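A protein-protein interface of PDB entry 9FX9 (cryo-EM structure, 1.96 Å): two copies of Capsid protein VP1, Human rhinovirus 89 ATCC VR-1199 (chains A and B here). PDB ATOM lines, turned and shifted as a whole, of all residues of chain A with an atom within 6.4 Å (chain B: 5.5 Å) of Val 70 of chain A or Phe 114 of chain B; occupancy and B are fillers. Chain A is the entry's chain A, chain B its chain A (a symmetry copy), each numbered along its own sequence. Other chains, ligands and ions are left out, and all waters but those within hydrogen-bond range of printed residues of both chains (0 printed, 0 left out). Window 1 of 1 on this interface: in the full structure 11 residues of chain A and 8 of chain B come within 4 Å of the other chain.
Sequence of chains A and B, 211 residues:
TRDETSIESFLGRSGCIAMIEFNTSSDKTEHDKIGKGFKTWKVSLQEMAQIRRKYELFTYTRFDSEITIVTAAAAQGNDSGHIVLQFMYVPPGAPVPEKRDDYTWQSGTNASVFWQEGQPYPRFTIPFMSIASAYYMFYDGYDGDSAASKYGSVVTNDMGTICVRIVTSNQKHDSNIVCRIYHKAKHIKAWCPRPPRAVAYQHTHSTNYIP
CG1 of Val 70 of chain A touches CD2 of Phe 114 of chain B, 3.7 Å away.
CG1 of Val 167 of chain B touches CB of Ala 72 of chain A, 3.9 Å away.
Val 84 of chain B touches Tyr 121 of chain A (CG1 to OH, 3.1 Å).
Arg 180 of chain A touches Arg 165 of chain B.
Arg 180 of chain A touches Val 167 of chain B.
Phe 114 of chain B touches Tyr 182 of chain A.
The side-chain hydroxyl (OH) of Tyr 121 of chain A sits at hydrogen-bond distance from the side-chain amide oxygen (OE1) of Gln 116 of chain B.
No position is printed for both chains.
N of Arg 180 of chain A sits at hydrogen-bond distance from O of Val 70 of chain A, at 2.8 Å.
The side-chain amide oxygen (OE1) of Gln 86 of chain B is in hydrogen-bond range of the guanidinium group (NE) of Arg 165 of chain B (2.9 Å).
The backbone carbonyl oxygen of Ala 72 of chain A is in hydrogen-bond range of the backbone NH of Val 178 of chain A (2.9 Å).
O of Thr 68 of chain A is in hydrogen-bond range of N of Tyr 182 of chain A, at 2.9 Å.
The backbone NH of Gln 116 of chain B lies within hydrogen-bond range of the side-chain amide oxygen of Gln 119 of chain B, 3.3 Å away.
The backbone NH of Val 167 of chain B sits at hydrogen-bond distance from the backbone carbonyl oxygen of Val 84 of chain B (2.9 Å).
Printed residues of chain B within 4 Å of Val 70 of chain A: Phe 114.
Phe 114 of chain B touches just these residues of chain A: Val 70 (3.7 Å) and Tyr 182 (3.0 Å).
Printed residues of chain B within 4 Å of Tyr 182 of chain A: Phe 114.
Of the printed residues of chain A, Val 167 of chain B touches Ala 72 and Arg 180.
Phe 87 of chain B touches none of the printed residues of chain A.
The nearest residue of chain A that does not touch Phe 114 of chain B is Tyr 121 of chain A (4.02 Å).
The nearest printed residue of chain A that does not touch Gln 116 of chain B is Thr 71 of chain A (5.2 Å).
Of the 12 printed residues of chain B, 5 touch a printed residue of chain A.
Hydrophobic or aromatic side chains of chain B that line the printed part of chain A: Val 84, Phe 114 and Val 167.
Hydrophobic or aromatic side chains of chain A within 4 Å of the printed part of chain B: Val 70, Ala 72, Tyr 121 and Tyr 182.
Along chain A the printed residues that touch a printed residue of chain B span positions 70 to 182.
Among the printed residues, 7 pairs touch across the chains.
Among the printed residues, no Asp or Glu carboxylate lies within 4 Å of a Lys or Arg side-chain nitrogen of the other chain.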
ATOM      1  N   THR A  68       7.682  15.026  23.898  1.00  0.00           N
ATOM      2  CA  THR A  68       7.654  16.491  23.954  1.00  0.00           C
ATOM      3  C   THR A  68       7.855  16.904  25.399  1.00  0.00           C
ATOM      4  O   THR A  68       7.163  16.386  26.267  1.00  0.00           O
ATOM      5  CB  THR A  68       6.333  17.059  23.420  1.00  0.00           C
ATOM      6  OG1 THR A  68       6.048  16.523  22.146  1.00  0.00           O
ATOM      7  CG2 THR A  68       6.363  18.576  23.284  1.00  0.00           C
ATOM      8  N   ILE A  69       8.787  17.804  25.697  1.00  0.00           N
ATOM      9  CA  ILE A  69       9.095  18.141  27.094  1.00  0.00           C
ATOM     10  C   ILE A  69       8.650  19.564  27.394  1.00  0.00           C
ATOM     11  O   ILE A  69       9.243  20.524  26.911  1.00  0.00           O
ATOM     12  CB  ILE A  69      10.577  17.874  27.435  1.00  0.00           C
ATOM     13  CG1 ILE A  69      11.017  16.473  26.958  1.00  0.00           C
ATOM     14  CG2 ILE A  69      10.763  18.029  28.947  1.00  0.00           C
ATOM     15  CD1 ILE A  69      12.480  16.113  27.226  1.00  0.00           C
ATOM     16  N   VAL A  70       7.622  19.721  28.223  1.00  0.00           N
ATOM     17  CA  VAL A  70       7.133  21.038  28.653  1.00  0.00           C
ATOM     18  C   VAL A  70       7.861  21.427  29.925  1.00  0.00           C
ATOM     19  O   VAL A  70       7.705  20.782  30.956  1.00  0.00           O
ATOM     20  CB  VAL A  70       5.610  21.052  28.853  1.00  0.00           C
ATOM     21  CG1 VAL A  70       5.101  22.378  29.426  1.00  0.00           C
ATOM     22  CG2 VAL A  70       4.903  20.799  27.529  1.00  0.00           C
ATOM     23  N   THR A  71       8.659  22.482  29.857  1.00  0.00           N
ATOM     24  CA  THR A  71       9.476  22.946  30.984  1.00  0.00           C
ATOM     25  C   THR A  71       8.984  24.270  31.541  1.00  0.00           C
ATOM     26  O   THR A  71       8.795  25.229  30.797  1.00  0.00           O
ATOM     27  CB  THR A  71      10.948  23.052  30.592  1.00  0.00           C
ATOM     28  OG1 THR A  71      11.402  21.773  30.230  1.00  0.00           O
ATOM     29  CG2 THR A  71      11.824  23.541  31.742  1.00  0.00           C
ATOM     30  N   ALA A  72       8.856  24.344  32.861  1.00  0.00           N
ATOM     31  CA  ALA A  72       8.721  25.582  33.614  1.00  0.00           C
ATOM     32  C   ALA A  72       9.868  25.700  34.627  1.00  0.00           C
ATOM     33  O   ALA A  72      10.309  24.700  35.197  1.00  0.00           O
ATOM     34  CB  ALA A  72       7.345  25.601  34.282  1.00  0.00           C
ATOM     35  N   TYR A 121       8.843  24.154  22.571  1.00  0.00           N
ATOM     36  CA  TYR A 121       9.255  23.007  23.383  1.00  0.00           C
ATOM     37  C   TYR A 121       9.951  21.917  22.558  1.00  0.00           C
ATOM     38  O   TYR A 121       9.552  21.655  21.423  1.00  0.00           O
ATOM     39  CB  TYR A 121       8.062  22.446  24.162  1.00  0.00           C
ATOM     40  CG  TYR A 121       7.607  23.368  25.272  1.00  0.00           C
ATOM     41  CD1 TYR A 121       8.505  23.732  26.293  1.00  0.00           C
ATOM     42  CD2 TYR A 121       6.304  23.890  25.263  1.00  0.00           C
ATOM     43  CE1 TYR A 121       8.108  24.636  27.291  1.00  0.00           C
ATOM     44  CE2 TYR A 121       5.898  24.781  26.273  1.00  0.00           C
ATOM     45  CZ  TYR A 121       6.803  25.162  27.282  1.00  0.00           C
ATOM     46  OH  TYR A 121       6.422  26.040  28.242  1.00  0.00           O
ATOM     47  N   PRO A 122      10.991  21.267  23.107  1.00  0.00           N
ATOM     48  CA  PRO A 122      11.776  20.289  22.380  1.00  0.00           C
ATOM     49  C   PRO A 122      10.952  19.032  22.118  1.00  0.00           C
ATOM     50  O   PRO A 122      10.206  18.563  22.980  1.00  0.00           O
ATOM     51  CB  PRO A 122      13.005  20.021  23.241  1.00  0.00           C
ATOM     52  CG  PRO A 122      12.507  20.285  24.654  1.00  0.00           C
ATOM     53  CD  PRO A 122      11.480  21.393  24.465  1.00  0.00           C
ATOM     54  N   VAL A 178      10.902  22.270  36.615  1.00  0.00           N
ATOM     55  CA  VAL A 178       9.938  21.179  36.428  1.00  0.00           C
ATOM     56  C   VAL A 178       9.730  20.892  34.945  1.00  0.00           C
ATOM     57  O   VAL A 178       9.320  21.770  34.188  1.00  0.00           O
ATOM     58  CB  VAL A 178       8.591  21.476  37.111  1.00  0.00           C
ATOM     59  CG1 VAL A 178       7.607  20.312  36.938  1.00  0.00           C
ATOM     60  CG2 VAL A 178       8.753  21.717  38.612  1.00  0.00           C
ATOM     61  N   CYS A 179       9.950  19.646  34.535  1.00  0.00           N
ATOM     62  CA  CYS A 179       9.763  19.166  33.171  1.00  0.00           C
ATOM     63  C   CYS A 179       8.673  18.086  33.121  1.00  0.00           C
ATOM     64  O   CYS A 179       8.843  16.985  33.645  1.00  0.00           O
ATOM     65  CB  CYS A 179      11.100  18.629  32.641  1.00  0.00           C
ATOM     66  SG  CYS A 179      12.392  19.896  32.704  1.00  0.00           S
ATOM     67  N   ARG A 180       7.568  18.380  32.433  1.00  0.00           N
ATOM     68  CA  ARG A 180       6.499  17.432  32.109  1.00  0.00           C
ATOM     69  C   ARG A 180       6.876  16.693  30.837  1.00  0.00           C
ATOM     70  O   ARG A 180       7.022  17.314  29.786  1.00  0.00           O
ATOM     71  CB  ARG A 180       5.178  18.181  31.907  1.00  0.00           C
ATOM     72  CG  ARG A 180       4.598  18.732  33.206  1.00  0.00           C
ATOM     73  CD  ARG A 180       3.495  19.762  32.946  1.00  0.00           C
ATOM     74  NE  ARG A 180       2.904  20.229  34.211  1.00  0.00           N
ATOM     75  CZ  ARG A 180       3.414  21.081  35.076  1.00  0.00           C
ATOM     76  NH1 ARG A 180       2.792  21.335  36.187  1.00  0.00           N
ATOM     77  NH2 ARG A 180       4.539  21.695  34.863  1.00  0.00           N
ATOM     78  N   ILE A 181       7.043  15.384  30.915  1.00  0.00           N
ATOM     79  CA  ILE A 181       7.384  14.551  29.764  1.00  0.00           C
ATOM     80  C   ILE A 181       6.084  14.064  29.136  1.00  0.00           C
ATOM     81  O   ILE A 181       5.461  13.121  29.618  1.00  0.00           O
ATOM     82  CB  ILE A 181       8.349  13.426  30.184  1.00  0.00           C
ATOM     83  CG1 ILE A 181       9.687  14.057  30.622  1.00  0.00           C
ATOM     84  CG2 ILE A 181       8.586  12.415  29.052  1.00  0.00           C
ATOM     85  CD1 ILE A 181      10.645  13.083  31.300  1.00  0.00           C
ATOM     86  N   TYR A 182       5.656  14.730  28.072  1.00  0.00           N
ATOM     87  CA  TYR A 182       4.549  14.266  27.258  1.00  0.00           C
ATOM     88  C   TYR A 182       5.036  13.207  26.283  1.00  0.00           C
ATOM     89  O   TYR A 182       6.037  13.385  25.596  1.00  0.00           O
ATOM     90  CB  TYR A 182       3.853  15.422  26.543  1.00  0.00           C
ATOM     91  CG  TYR A 182       2.922  16.188  27.449  1.00  0.00           C
ATOM     92  CD1 TYR A 182       3.442  17.115  28.370  1.00  0.00           C
ATOM     93  CD2 TYR A 182       1.538  15.945  27.394  1.00  0.00           C
ATOM     94  CE1 TYR A 182       2.574  17.791  29.243  1.00  0.00           C
ATOM     95  CE2 TYR A 182       0.670  16.620  28.267  1.00  0.00           C
ATOM     96  CZ  TYR A 182       1.192  17.541  29.196  1.00  0.00           C
ATOM     97  OH  TYR A 182       0.362  18.188  30.053  1.00  0.00           O
ATOM     98  N   VAL B  84       4.383  30.804  31.617  1.00  0.00           N
ATOM     99  CA  VAL B  84       3.843  29.669  30.851  1.00  0.00           C
ATOM    100  C   VAL B  84       2.424  29.351  31.316  1.00  0.00           C
ATOM    101  O   VAL B  84       2.184  29.143  32.506  1.00  0.00           O
ATOM    102  CB  VAL B  84       4.741  28.424  30.952  1.00  0.00           C
ATOM    103  CG1 VAL B  84       4.216  27.282  30.074  1.00  0.00           C
ATOM    104  CG2 VAL B  84       6.175  28.731  30.519  1.00  0.00           C
ATOM    105  N   LEU B  85       1.487  29.275  30.374  1.00  0.00           N
ATOM    106  CA  LEU B  85       0.093  28.922  30.619  1.00  0.00           C
ATOM    107  C   LEU B  85      -0.287  27.637  29.886  1.00  0.00           C
ATOM    108  O   LEU B  85       0.178  27.373  28.780  1.00  0.00           O
ATOM    109  CB  LEU B  85      -0.846  30.055  30.181  1.00  0.00           C
ATOM    110  CG  LEU B  85      -0.614  31.422  30.836  1.00  0.00           C
ATOM    111  CD1 LEU B  85      -1.704  32.373  30.373  1.00  0.00           C
ATOM    112  CD2 LEU B  85      -0.662  31.377  32.358  1.00  0.00           C
ATOM    113  N   GLN B  86      -1.184  26.864  30.491  1.00  0.00           N
ATOM    114  CA  GLN B  86      -1.879  25.769  29.829  1.00  0.00           C
ATOM    115  C   GLN B  86      -3.333  26.181  29.611  1.00  0.00           C
ATOM    116  O   GLN B  86      -4.057  26.457  30.568  1.00  0.00           O
ATOM    117  CB  GLN B  86      -1.756  24.486  30.664  1.00  0.00           C
ATOM    118  CG  GLN B  86      -2.443  23.272  30.021  1.00  0.00           C
ATOM    119  CD  GLN B  86      -2.382  22.017  30.889  1.00  0.00           C
ATOM    120  OE1 GLN B  86      -1.784  21.985  31.956  1.00  0.00           O
ATOM    121  NE2 GLN B  86      -3.018  20.944  30.482  1.00  0.00           N
ATOM    122  N   PHE B  87      -3.768  26.169  28.354  1.00  0.00           N
ATOM    123  CA  PHE B  87      -5.164  26.319  27.967  1.00  0.00           C
ATOM    124  C   PHE B  87      -5.688  24.945  27.588  1.00  0.00           C
ATOM    125  O   PHE B  87      -5.110  24.277  26.736  1.00  0.00           O
ATOM    126  CB  PHE B  87      -5.294  27.269  26.774  1.00  0.00           C
ATOM    127  CG  PHE B  87      -4.786  28.661  27.050  1.00  0.00           C
ATOM    128  CD1 PHE B  87      -5.610  29.564  27.731  1.00  0.00           C
ATOM    129  CD2 PHE B  87      -3.499  29.053  26.645  1.00  0.00           C
ATOM    130  CE1 PHE B  87      -5.138  30.842  28.055  1.00  0.00           C
ATOM    131  CE2 PHE B  87      -3.035  30.345  26.948  1.00  0.00           C
ATOM    132  CZ  PHE B  87      -3.846  31.228  27.670  1.00  0.00           C
ATOM    133  N   SER B 112      -5.090  20.163  25.037  1.00  0.00           N
ATOM    134  CA  SER B 112      -4.332  21.242  25.684  1.00  0.00           C
ATOM    135  C   SER B 112      -3.396  21.931  24.704  1.00  0.00           C
ATOM    136  O   SER B 112      -2.730  21.278  23.906  1.00  0.00           O
ATOM    137  CB  SER B 112      -3.516  20.749  26.876  1.00  0.00           C
ATOM    138  OG  SER B 112      -4.361  20.378  27.935  1.00  0.00           O
ATOM    139  N   VAL B 113      -3.291  23.248  24.808  1.00  0.00           N
ATOM    140  CA  VAL B 113      -2.211  24.026  24.208  1.00  0.00           C
ATOM    141  C   VAL B 113      -1.422  24.715  25.313  1.00  0.00           C
ATOM    142  O   VAL B 113      -1.961  25.459  26.128  1.00  0.00           O
ATOM    143  CB  VAL B 113      -2.717  24.942  23.079  1.00  0.00           C
ATOM    144  CG1 VAL B 113      -3.779  25.952  23.496  1.00  0.00           C
ATOM    145  CG2 VAL B 113      -1.563  25.718  22.443  1.00  0.00           C
ATOM    146  N   PHE B 114      -0.128  24.430  25.365  1.00  0.00           N
ATOM    147  CA  PHE B 114       0.812  25.131  26.225  1.00  0.00           C
ATOM    148  C   PHE B 114       1.352  26.327  25.454  1.00  0.00           C
ATOM    149  O   PHE B 114       1.836  26.184  24.333  1.00  0.00           O
ATOM    150  CB  PHE B 114       1.939  24.196  26.672  1.00  0.00           C
ATOM    151  CG  PHE B 114       1.480  23.094  27.597  1.00  0.00           C
ATOM    152  CD1 PHE B 114       0.950  21.906  27.069  1.00  0.00           C
ATOM    153  CD2 PHE B 114       1.563  23.261  28.990  1.00  0.00           C
ATOM    154  CE1 PHE B 114       0.493  20.895  27.929  1.00  0.00           C
ATOM    155  CE2 PHE B 114       1.116  22.247  29.848  1.00  0.00           C
ATOM    156  CZ  PHE B 114       0.580  21.066  29.316  1.00  0.00           C
ATOM    157  N   TRP B 115       1.259  27.506  26.051  1.00  0.00           N
ATOM    158  CA  TRP B 115       1.684  28.764  25.455  1.00  0.00           C
ATOM    159  C   TRP B 115       2.578  29.512  26.427  1.00  0.00           C
ATOM    160  O   TRP B 115       2.339  29.513  27.633  1.00  0.00           O
ATOM    161  CB  TRP B 115       0.461  29.587  25.044  1.00  0.00           C
ATOM    162  CG  TRP B 115       0.742  30.980  24.571  1.00  0.00           C
ATOM    163  CD1 TRP B 115       1.103  31.327  23.316  1.00  0.00           C
ATOM    164  CD2 TRP B 115       0.748  32.221  25.341  1.00  0.00           C
ATOM    165  NE1 TRP B 115       1.280  32.695  23.245  1.00  0.00           N
ATOM    166  CE2 TRP B 115       1.064  33.295  24.460  1.00  0.00           C
ATOM    167  CE3 TRP B 115       0.523  32.555  26.694  1.00  0.00           C
ATOM    168  CZ2 TRP B 115       1.126  34.628  24.887  1.00  0.00           C
ATOM    169  CZ3 TRP B 115       0.591  33.889  27.136  1.00  0.00           C
ATOM    170  CH2 TRP B 115       0.880  34.925  26.233  1.00  0.00           C
ATOM    171  N   GLN B 116       3.618  30.147  25.906  1.00  0.00           N
ATOM    172  CA  GLN B 116       4.570  30.899  26.711  1.00  0.00           C
ATOM    173  C   GLN B 116       4.662  32.338  26.220  1.00  0.00           C
ATOM    174  O   GLN B 116       4.581  32.614  25.030  1.00  0.00           O
ATOM    175  CB  GLN B 116       5.904  30.150  26.812  1.00  0.00           C
ATOM    176  CG  GLN B 116       6.615  29.837  25.492  1.00  0.00           C
ATOM    177  CD  GLN B 116       7.616  28.690  25.630  1.00  0.00           C
ATOM    178  OE1 GLN B 116       8.116  28.369  26.699  1.00  0.00           O
ATOM    179  NE2 GLN B 116       7.960  28.020  24.558  1.00  0.00           N
ATOM    180  N   GLN B 119       5.265  34.495  22.607  1.00  0.00           N
ATOM    181  CA  GLN B 119       4.969  33.610  21.475  1.00  0.00           C
ATOM    182  C   GLN B 119       3.663  34.054  20.779  1.00  0.00           C
ATOM    183  O   GLN B 119       2.775  34.576  21.461  1.00  0.00           O
ATOM    184  CB  GLN B 119       4.868  32.190  22.053  1.00  0.00           C
ATOM    185  CG  GLN B 119       4.798  31.020  21.074  1.00  0.00           C
ATOM    186  CD  GLN B 119       4.828  29.693  21.834  1.00  0.00           C
ATOM    187  OE1 GLN B 119       4.000  29.414  22.691  1.00  0.00           O
ATOM    188  NE2 GLN B 119       5.783  28.827  21.571  1.00  0.00           N
ATOM    189  N   ARG B 165      -4.776  27.447  33.386  1.00  0.00           N
ATOM    190  CA  ARG B 165      -3.925  27.491  34.578  1.00  0.00           C
ATOM    191  C   ARG B 165      -2.546  28.035  34.255  1.00  0.00           C
ATOM    192  O   ARG B 165      -2.029  27.835  33.159  1.00  0.00           O
ATOM    193  CB  ARG B 165      -3.854  26.128  35.290  1.00  0.00           C
ATOM    194  CG  ARG B 165      -3.102  25.037  34.516  1.00  0.00           C
ATOM    195  CD  ARG B 165      -2.954  23.793  35.388  1.00  0.00           C
ATOM    196  NE  ARG B 165      -2.228  22.719  34.694  1.00  0.00           N
ATOM    197  CZ  ARG B 165      -1.644  21.675  35.244  1.00  0.00           C
ATOM    198  NH1 ARG B 165      -0.971  20.861  34.491  1.00  0.00           N
ATOM    199  NH2 ARG B 165      -1.714  21.429  36.519  1.00  0.00           N
ATOM    200  N   VAL B 167       1.298  27.404  34.666  1.00  0.00           N
ATOM    201  CA  VAL B 167       2.221  26.269  34.841  1.00  0.00           C
ATOM    202  C   VAL B 167       3.424  26.668  35.707  1.00  0.00           C
ATOM    203  O   VAL B 167       3.887  25.880  36.526  1.00  0.00           O
ATOM    204  CB  VAL B 167       2.679  25.744  33.469  1.00  0.00           C
ATOM    205  CG1 VAL B 167       3.661  24.576  33.578  1.00  0.00           C
ATOM    206  CG2 VAL B 167       1.490  25.266  32.632  1.00  0.00           C
